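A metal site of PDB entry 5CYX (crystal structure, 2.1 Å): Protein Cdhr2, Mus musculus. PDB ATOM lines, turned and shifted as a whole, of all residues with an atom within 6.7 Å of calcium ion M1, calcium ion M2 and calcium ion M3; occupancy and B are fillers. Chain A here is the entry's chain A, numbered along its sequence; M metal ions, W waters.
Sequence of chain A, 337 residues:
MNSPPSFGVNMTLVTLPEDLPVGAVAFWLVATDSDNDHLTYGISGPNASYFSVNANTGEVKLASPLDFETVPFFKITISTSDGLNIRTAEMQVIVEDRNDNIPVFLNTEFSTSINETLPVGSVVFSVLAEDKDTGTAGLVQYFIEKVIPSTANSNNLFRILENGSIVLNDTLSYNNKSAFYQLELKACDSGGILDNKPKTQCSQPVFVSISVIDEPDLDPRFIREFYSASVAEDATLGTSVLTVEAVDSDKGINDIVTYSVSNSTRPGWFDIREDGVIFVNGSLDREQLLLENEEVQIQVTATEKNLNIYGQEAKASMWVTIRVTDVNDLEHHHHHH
Calcium ion M3 is bound by OD2 of Asp 100 (2.2 Å), OD1 of Asp 67 (2.3 Å), OE1 of Glu 18 (2.4 Å), OE1 of Glu 69 (2.4 Å) and water W1 (2.5 Å).
Calcium ion M1 is bound by OD1 of Asn 99 (2.3 Å).
The side-chain carboxylate (OD2) of Asp 131 binds calcium ion M1 (2.3 Å).
O of Asn 101 is bound to calcium ion M1 (2.3 Å).
OD2 of Asp 133 binds calcium ion M1 (2.3 Å).
The backbone carbonyl oxygen (O) of Ala 137 binds calcium ion M1 (2.3 Å).
OD2 of Asp 189 is bound to calcium ion M1, at 2.5 Å.
Calcium ion M1 is bound by OD1 of Asp 131, 2.5 Å away.
Calcium ion M2 is bound by OE2 of Glu 18 (2.2 Å), OD1 of Asp 97 (2.3 Å), OD1 of Asp 100 (2.4 Å), OD1 of Asp 133 (2.4 Å), O of Arg 98 (2.4 Å), OE2 of Glu 69 (2.5 Å) and OE1 of Glu 69 (2.7 Å).
Calcium ion M2 has seven donor atoms within binding distance.
Of the 26 residues printed, 7 come within 4 Å of calcium ion M2.
Four residues have an atom within 4 Å of calcium ion M3: Glu 18, Asp 67, Glu 69 and Asp 100.
Along chain A the residues within 4 Å of calcium ion M3 span positions 18 to 100.
The nearest printed residue that does not touch calcium ion M3 is Phe 68 (4.2 Å).
N of Glu 18 sits at hydrogen-bond distance from O of Glu 96, at 3.1 Å.
The side-chain carboxylate (OD2) of Asp 67 lies within hydrogen-bond range of the side-chain hydroxyl (OG1) of Thr 70 (2.6 Å).
The backbone carbonyl oxygen of Asn 99 lies within hydrogen-bond range of the side-chain amide nitrogen of Gln 201 (3.1 Å).
NH1 of Arg 98 lies within salt-bridge range of OE1 of Glu 96 (3.1 Å).
The side-chain amide nitrogen (ND2) of Asn 101 sits close to the side-chain carboxylate (OE1) of Glu 69, 3.4 Å away.
OD1 of Asp 189 lies within hydrogen-bond range of N of Gln 201 (2.9 Å).
OD1 of Asp 100 lies close to ND2 of Asn 101, 3.3 Å away.
The side-chain carboxylate of Glu 18 sits close to the backbone NH of Phe 68 (2.9 Å).
The nearest printed residue that does not touch calcium ion M1 is Ile 102 (4.4 Å).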
ATOM      1  N   GLU A  18      29.205 -13.332  -6.562  1.00  0.00           N
ATOM      2  CA  GLU A  18      29.050 -12.527  -7.760  1.00  0.00           C
ATOM      3  C   GLU A  18      30.358 -11.842  -8.201  1.00  0.00           C
ATOM      4  O   GLU A  18      30.486 -11.495  -9.306  1.00  0.00           O
ATOM      5  CB  GLU A  18      27.918 -11.507  -7.583  1.00  0.00           C
ATOM      6  CG  GLU A  18      28.182 -10.292  -6.691  1.00  0.00           C
ATOM      7  CD  GLU A  18      27.204  -9.154  -6.919  1.00  0.00           C
ATOM      8  OE1 GLU A  18      26.766  -8.918  -8.099  1.00  0.00           O
ATOM      9  OE2 GLU A  18      26.876  -8.428  -5.943  1.00  0.00           O
ATOM     10  N   LEU A  66      28.995 -12.875 -13.409  1.00  0.00           N
ATOM     11  CA  LEU A  66      27.888 -13.048 -12.534  1.00  0.00           C
ATOM     12  C   LEU A  66      27.499 -11.689 -12.001  1.00  0.00           C
ATOM     13  O   LEU A  66      28.367 -10.835 -11.823  1.00  0.00           O
ATOM     14  CB  LEU A  66      28.311 -13.898 -11.322  1.00  0.00           C
ATOM     15  CG  LEU A  66      28.666 -15.352 -11.567  1.00  0.00           C
ATOM     16  CD1 LEU A  66      29.060 -16.025 -10.258  1.00  0.00           C
ATOM     17  CD2 LEU A  66      27.506 -16.109 -12.185  1.00  0.00           C
ATOM     18  N   ASP A  67      26.215 -11.522 -11.683  1.00  0.00           N
ATOM     19  CA  ASP A  67      25.735 -10.230 -11.224  1.00  0.00           C
ATOM     20  C   ASP A  67      24.447 -10.440 -10.459  1.00  0.00           C
ATOM     21  O   ASP A  67      23.379 -10.663 -11.039  1.00  0.00           O
ATOM     22  CB  ASP A  67      25.494  -9.257 -12.436  1.00  0.00           C
ATOM     23  CG  ASP A  67      25.054  -7.865 -11.976  1.00  0.00           C
ATOM     24  OD1 ASP A  67      25.223  -7.486 -10.790  1.00  0.00           O
ATOM     25  OD2 ASP A  67      24.490  -7.134 -12.768  1.00  0.00           O
ATOM     26  N   PHE A  68      24.549 -10.385  -9.142  1.00  0.00           N
ATOM     27  CA  PHE A  68      23.444 -10.590  -8.271  1.00  0.00           C
ATOM     28  C   PHE A  68      22.322  -9.610  -8.548  1.00  0.00           C
ATOM     29  O   PHE A  68      21.161  -9.982  -8.499  1.00  0.00           O
ATOM     30  CB  PHE A  68      23.876 -10.397  -6.815  1.00  0.00           C
ATOM     31  CG  PHE A  68      22.759 -10.573  -5.850  1.00  0.00           C
ATOM     32  CD1 PHE A  68      22.333 -11.842  -5.497  1.00  0.00           C
ATOM     33  CD2 PHE A  68      22.108  -9.471  -5.287  1.00  0.00           C
ATOM     34  CE1 PHE A  68      21.307 -12.009  -4.572  1.00  0.00           C
ATOM     35  CE2 PHE A  68      21.082  -9.633  -4.375  1.00  0.00           C
ATOM     36  CZ  PHE A  68      20.674 -10.898  -4.050  1.00  0.00           C
ATOM     37  N   GLU A  69      22.682  -8.365  -8.859  1.00  0.00           N
ATOM     38  CA  GLU A  69      21.678  -7.328  -9.073  1.00  0.00           C
ATOM     39  C   GLU A  69      20.720  -7.619 -10.250  1.00  0.00           C
ATOM     40  O   GLU A  69      19.558  -7.156 -10.210  1.00  0.00           O
ATOM     41  CB  GLU A  69      22.336  -5.961  -9.260  1.00  0.00           C
ATOM     42  CG  GLU A  69      22.740  -5.298  -7.959  1.00  0.00           C
ATOM     43  CD  GLU A  69      23.806  -6.067  -7.158  1.00  0.00           C
ATOM     44  OE1 GLU A  69      24.870  -6.436  -7.650  1.00  0.00           O
ATOM     45  OE2 GLU A  69      23.600  -6.334  -6.002  1.00  0.00           O
ATOM     46  N   THR A  70      21.152  -8.391 -11.255  1.00  0.00           N
ATOM     47  CA  THR A  70      20.274  -8.782 -12.392  1.00  0.00           C
ATOM     48  C   THR A  70      19.851 -10.247 -12.408  1.00  0.00           C
ATOM     49  O   THR A  70      18.697 -10.539 -12.692  1.00  0.00           O
ATOM     50  CB  THR A  70      20.910  -8.486 -13.750  1.00  0.00           C
ATOM     51  OG1 THR A  70      22.315  -8.351 -13.555  1.00  0.00           O
ATOM     52  CG2 THR A  70      20.406  -7.203 -14.339  1.00  0.00           C
ATOM     53  N   GLU A  96      25.616 -15.220  -4.865  1.00  0.00           N
ATOM     54  CA  GLU A  96      25.633 -14.416  -3.637  1.00  0.00           C
ATOM     55  C   GLU A  96      26.000 -12.950  -3.879  1.00  0.00           C
ATOM     56  O   GLU A  96      26.973 -12.617  -4.607  1.00  0.00           O
ATOM     57  CB  GLU A  96      26.618 -14.978  -2.623  1.00  0.00           C
ATOM     58  CG  GLU A  96      26.167 -16.237  -1.927  1.00  0.00           C
ATOM     59  CD  GLU A  96      27.022 -16.575  -0.696  1.00  0.00           C
ATOM     60  OE1 GLU A  96      28.248 -16.288  -0.730  1.00  0.00           O
ATOM     61  OE2 GLU A  96      26.433 -17.145   0.271  1.00  0.00           O
ATOM     62  N   ASP A  97      25.269 -12.086  -3.189  1.00  0.00           N
ATOM     63  CA  ASP A  97      25.473 -10.653  -3.237  1.00  0.00           C
ATOM     64  C   ASP A  97      26.849 -10.317  -2.650  1.00  0.00           C
ATOM     65  O   ASP A  97      27.267 -10.913  -1.622  1.00  0.00           O
ATOM     66  CB  ASP A  97      24.369  -9.913  -2.432  1.00  0.00           C
ATOM     67  CG  ASP A  97      24.353  -8.393  -2.719  1.00  0.00           C
ATOM     68  OD1 ASP A  97      24.868  -7.943  -3.780  1.00  0.00           O
ATOM     69  OD2 ASP A  97      23.867  -7.639  -1.828  1.00  0.00           O
ATOM     70  N   ARG A  98      27.556  -9.408  -3.327  1.00  0.00           N
ATOM     71  CA  ARG A  98      28.787  -8.781  -2.717  1.00  0.00           C
ATOM     72  C   ARG A  98      28.681  -7.242  -2.856  1.00  0.00           C
ATOM     73  O   ARG A  98      27.878  -6.700  -3.698  1.00  0.00           O
ATOM     74  CB  ARG A  98      30.023  -9.334  -3.380  1.00  0.00           C
ATOM     75  CG  ARG A  98      30.283 -10.811  -3.129  1.00  0.00           C
ATOM     76  CD  ARG A  98      30.979 -10.976  -1.808  1.00  0.00           C
ATOM     77  NE  ARG A  98      31.193 -12.365  -1.442  1.00  0.00           N
ATOM     78  CZ  ARG A  98      30.327 -13.161  -0.841  1.00  0.00           C
ATOM     79  NH1 ARG A  98      30.673 -14.395  -0.549  1.00  0.00           N
ATOM     80  NH2 ARG A  98      29.107 -12.757  -0.515  1.00  0.00           N
ATOM     81  N   ASN A  99      29.433  -6.520  -2.029  1.00  0.00           N
ATOM     82  CA  ASN A  99      29.357  -5.079  -2.030  1.00  0.00           C
ATOM     83  C   ASN A  99      30.139  -4.441  -3.201  1.00  0.00           C
ATOM     84  O   ASN A  99      31.251  -3.887  -3.001  1.00  0.00           O
ATOM     85  CB  ASN A  99      29.809  -4.496  -0.713  1.00  0.00           C
ATOM     86  CG  ASN A  99      29.422  -3.082  -0.538  1.00  0.00           C
ATOM     87  OD1 ASN A  99      28.655  -2.536  -1.331  1.00  0.00           O
ATOM     88  ND2 ASN A  99      29.958  -2.469   0.468  1.00  0.00           N
ATOM     89  N   ASP A 100      29.545  -4.535  -4.398  1.00  0.00           N
ATOM     90  CA  ASP A 100      30.124  -3.940  -5.622  1.00  0.00           C
ATOM     91  C   ASP A 100      29.320  -2.732  -6.074  1.00  0.00           C
ATOM     92  O   ASP A 100      29.591  -2.226  -7.130  1.00  0.00           O
ATOM     93  CB  ASP A 100      30.155  -4.971  -6.768  1.00  0.00           C
ATOM     94  CG  ASP A 100      28.730  -5.566  -7.084  1.00  0.00           C
ATOM     95  OD1 ASP A 100      27.793  -5.416  -6.285  1.00  0.00           O
ATOM     96  OD2 ASP A 100      28.534  -6.155  -8.146  1.00  0.00           O
ATOM     97  N   ASN A 101      28.277  -2.280  -5.339  1.00  0.00           N
ATOM     98  CA  ASN A 101      27.650  -1.004  -5.768  1.00  0.00           C
ATOM     99  C   ASN A 101      27.880   0.114  -4.762  1.00  0.00           C
ATOM    100  O   ASN A 101      28.073  -0.178  -3.572  1.00  0.00           O
ATOM    101  CB  ASN A 101      26.179  -1.156  -6.091  1.00  0.00           C
ATOM    102  CG  ASN A 101      25.953  -1.890  -7.383  1.00  0.00           C
ATOM    103  OD1 ASN A 101      26.109  -1.317  -8.477  1.00  0.00           O
ATOM    104  ND2 ASN A 101      25.604  -3.149  -7.296  1.00  0.00           N
ATOM    105  N   ILE A 102      27.927   1.361  -5.278  1.00  0.00           N
ATOM    106  CA  ILE A 102      28.000   2.568  -4.433  1.00  0.00           C
ATOM    107  C   ILE A 102      26.641   3.293  -4.247  1.00  0.00           C
ATOM    108  O   ILE A 102      25.727   3.184  -5.096  1.00  0.00           O
ATOM    109  CB  ILE A 102      29.025   3.600  -4.909  1.00  0.00           C
ATOM    110  CG1 ILE A 102      28.642   4.187  -6.303  1.00  0.00           C
ATOM    111  CG2 ILE A 102      30.425   3.000  -5.039  1.00  0.00           C
ATOM    112  CD1 ILE A 102      29.573   5.321  -6.714  1.00  0.00           C
ATOM    113  N   PRO A 103      26.541   4.080  -3.157  1.00  0.00           N
ATOM    114  CA  PRO A 103      25.409   4.956  -2.982  1.00  0.00           C
ATOM    115  C   PRO A 103      25.439   6.047  -4.020  1.00  0.00           C
ATOM    116  O   PRO A 103      26.462   6.682  -4.201  1.00  0.00           O
ATOM    117  CB  PRO A 103      25.665   5.554  -1.598  1.00  0.00           C
ATOM    118  CG  PRO A 103      26.428   4.508  -0.865  1.00  0.00           C
ATOM    119  CD  PRO A 103      27.360   4.001  -1.936  1.00  0.00           C
ATOM    120  N   ASP A 131      21.612   2.653  -2.947  1.00  0.00           N
ATOM    121  CA  ASP A 131      22.693   1.720  -3.190  1.00  0.00           C
ATOM    122  C   ASP A 131      22.036   0.420  -3.545  1.00  0.00           C
ATOM    123  O   ASP A 131      21.270  -0.118  -2.752  1.00  0.00           O
ATOM    124  CB  ASP A 131      23.547   1.570  -1.927  1.00  0.00           C
ATOM    125  CG  ASP A 131      24.761   0.671  -2.123  1.00  0.00           C
ATOM    126  OD1 ASP A 131      24.669  -0.444  -2.662  1.00  0.00           O
ATOM    127  OD2 ASP A 131      25.862   1.039  -1.638  1.00  0.00           O
ATOM    128  N   LYS A 132      22.359  -0.100  -4.723  1.00  0.00           N
ATOM    129  CA  LYS A 132      21.674  -1.288  -5.255  1.00  0.00           C
ATOM    130  C   LYS A 132      21.971  -2.615  -4.569  1.00  0.00           C
ATOM    131  O   LYS A 132      21.257  -3.575  -4.812  1.00  0.00           O
ATOM    132  CB  LYS A 132      21.959  -1.420  -6.734  1.00  0.00           C
ATOM    133  CG  LYS A 132      21.361  -0.253  -7.506  1.00  0.00           C
ATOM    134  CD  LYS A 132      20.560  -0.746  -8.694  1.00  0.00           C
ATOM    135  CE  LYS A 132      21.453  -1.180  -9.844  1.00  0.00           C
ATOM    136  NZ  LYS A 132      20.835  -2.284 -10.668  1.00  0.00           N
ATOM    137  N   ASP A 133      22.987  -2.679  -3.706  1.00  0.00           N
ATOM    138  CA  ASP A 133      23.276  -3.933  -3.045  1.00  0.00           C
ATOM    139  C   ASP A 133      22.165  -4.171  -1.998  1.00  0.00           C
ATOM    140  O   ASP A 133      21.353  -3.298  -1.730  1.00  0.00           O
ATOM    141  CB  ASP A 133      24.688  -3.955  -2.418  1.00  0.00           C
ATOM    142  CG  ASP A 133      25.779  -3.666  -3.469  1.00  0.00           C
ATOM    143  OD1 ASP A 133      25.728  -4.285  -4.568  1.00  0.00           O
ATOM    144  OD2 ASP A 133      26.547  -2.756  -3.198  1.00  0.00           O
ATOM    145  N   THR A 134      22.176  -5.384  -1.436  1.00  0.00           N
ATOM    146  CA  THR A 134      21.174  -5.837  -0.467  1.00  0.00           C
ATOM    147  C   THR A 134      21.857  -6.083   0.884  1.00  0.00           C
ATOM    148  O   THR A 134      23.026  -6.441   0.929  1.00  0.00           O
ATOM    149  CB  THR A 134      20.571  -7.152  -0.977  1.00  0.00           C
ATOM    150  OG1 THR A 134      19.876  -6.914  -2.225  1.00  0.00           O
ATOM    151  CG2 THR A 134      19.548  -7.759   0.062  1.00  0.00           C
ATOM    152  N   THR A 136      23.519  -4.990   4.582  1.00  0.00           N
ATOM    153  CA  THR A 136      24.266  -3.817   5.057  1.00  0.00           C
ATOM    154  C   THR A 136      25.042  -3.220   3.901  1.00  0.00           C
ATOM    155  O   THR A 136      25.362  -2.045   3.925  1.00  0.00           O
ATOM    156  CB  THR A 136      25.220  -4.132   6.217  1.00  0.00           C
ATOM    157  OG1 THR A 136      26.146  -5.109   5.785  1.00  0.00           O
ATOM    158  CG2 THR A 136      24.391  -4.728   7.447  1.00  0.00           C
ATOM    159  N   ALA A 137      25.369  -4.017   2.906  1.00  0.00           N
ATOM    160  CA  ALA A 137      26.017  -3.477   1.709  1.00  0.00           C
ATOM    161  C   ALA A 137      25.142  -2.503   0.961  1.00  0.00           C
ATOM    162  O   ALA A 137      25.626  -1.758   0.063  1.00  0.00           O
ATOM    163  CB  ALA A 137      26.391  -4.607   0.785  1.00  0.00           C
ATOM    164  N   GLY A 138      23.820  -2.559   1.223  1.00  0.00           N
ATOM    165  CA  GLY A 138      22.880  -1.654   0.605  1.00  0.00           C
ATOM    166  C   GLY A 138      22.341  -0.546   1.485  1.00  0.00           C
ATOM    167  O   GLY A 138      21.577   0.273   1.037  1.00  0.00           O
ATOM    168  N   LEU A 139      22.764  -0.501   2.733  1.00  0.00           N
ATOM    169  CA  LEU A 139      22.144   0.305   3.761  1.00  0.00           C
ATOM    170  C   LEU A 139      22.965   1.600   3.876  1.00  0.00           C
ATOM    171  O   LEU A 139      24.157   1.585   4.362  1.00  0.00           O
ATOM    172  CB  LEU A 139      22.184  -0.457   5.077  1.00  0.00           C
ATOM    173  CG  LEU A 139      21.400   0.148   6.242  1.00  0.00           C
ATOM    174  CD1 LEU A 139      19.927   0.317   5.858  1.00  0.00           C
ATOM    175  CD2 LEU A 139      21.521  -0.763   7.459  1.00  0.00           C
ATOM    176  N   ASP A 189      27.719   3.078   2.303  1.00  0.00           N
ATOM    177  CA  ASP A 189      26.930   1.972   2.752  1.00  0.00           C
ATOM    178  C   ASP A 189      27.486   1.572   4.145  1.00  0.00           C
ATOM    179  O   ASP A 189      28.484   2.157   4.648  1.00  0.00           O
ATOM    180  CB  ASP A 189      26.866   0.827   1.718  1.00  0.00           C
ATOM    181  CG  ASP A 189      28.216   0.304   1.305  1.00  0.00           C
ATOM    182  OD1 ASP A 189      29.121   0.280   2.149  1.00  0.00           O
ATOM    183  OD2 ASP A 189      28.394  -0.039   0.099  1.00  0.00           O
ATOM    184  N   SER A 190      26.905   0.547   4.699  1.00  0.00           N
ATOM    185  CA  SER A 190      27.207   0.093   6.058  1.00  0.00           C
ATOM    186  C   SER A 190      28.136  -1.142   5.997  1.00  0.00           C
ATOM    187  O   SER A 190      28.278  -1.877   6.934  1.00  0.00           O
ATOM    188  CB  SER A 190      25.882  -0.216   6.791  1.00  0.00           C
ATOM    189  OG  SER A 190      24.970   0.878   6.768  1.00  0.00           O
ATOM    190  N   THR A 200      33.547  -1.194   2.382  1.00  0.00           N
ATOM    191  CA  THR A 200      32.507  -0.165   2.520  1.00  0.00           C
ATOM    192  C   THR A 200      32.613   0.700   1.285  1.00  0.00           C
ATOM    193  O   THR A 200      33.732   1.058   0.911  1.00  0.00           O
ATOM    194  CB  THR A 200      32.748   0.700   3.770  1.00  0.00           C
ATOM    195  OG1 THR A 200      32.570  -0.096   4.968  1.00  0.00           O
ATOM    196  CG2 THR A 200      31.807   1.915   3.785  1.00  0.00           C
ATOM    197  N   GLN A 201      31.494   1.049   0.648  1.00  0.00           N
ATOM    198  CA  GLN A 201      31.566   1.947  -0.553  1.00  0.00           C
ATOM    199  C   GLN A 201      31.025   3.321  -0.246  1.00  0.00           C
ATOM    200  O   GLN A 201      30.050   3.440   0.517  1.00  0.00           O
ATOM    201  CB  GLN A 201      30.794   1.352  -1.711  1.00  0.00           C
ATOM    202  CG  GLN A 201      31.234  -0.038  -2.118  1.00  0.00           C
ATOM    203  CD  GLN A 201      32.342  -0.052  -3.147  1.00  0.00           C
ATOM    204  OE1 GLN A 201      32.906   0.988  -3.484  1.00  0.00           O
ATOM    205  NE2 GLN A 201      32.644  -1.226  -3.651  1.00  0.00           N
HETATM  206 CA    CA M   1      26.964  -1.007  -1.705  1.00  0.00          CA
HETATM  207 CA    CA M   2      25.997  -6.536  -5.246  1.00  0.00          CA
HETATM  208 CA    CA M   3      26.719  -6.793  -9.179  1.00  0.00          CA
HETATM  209  O   HOH W   1      26.696  -4.494 -10.048  1.00  0.00           O
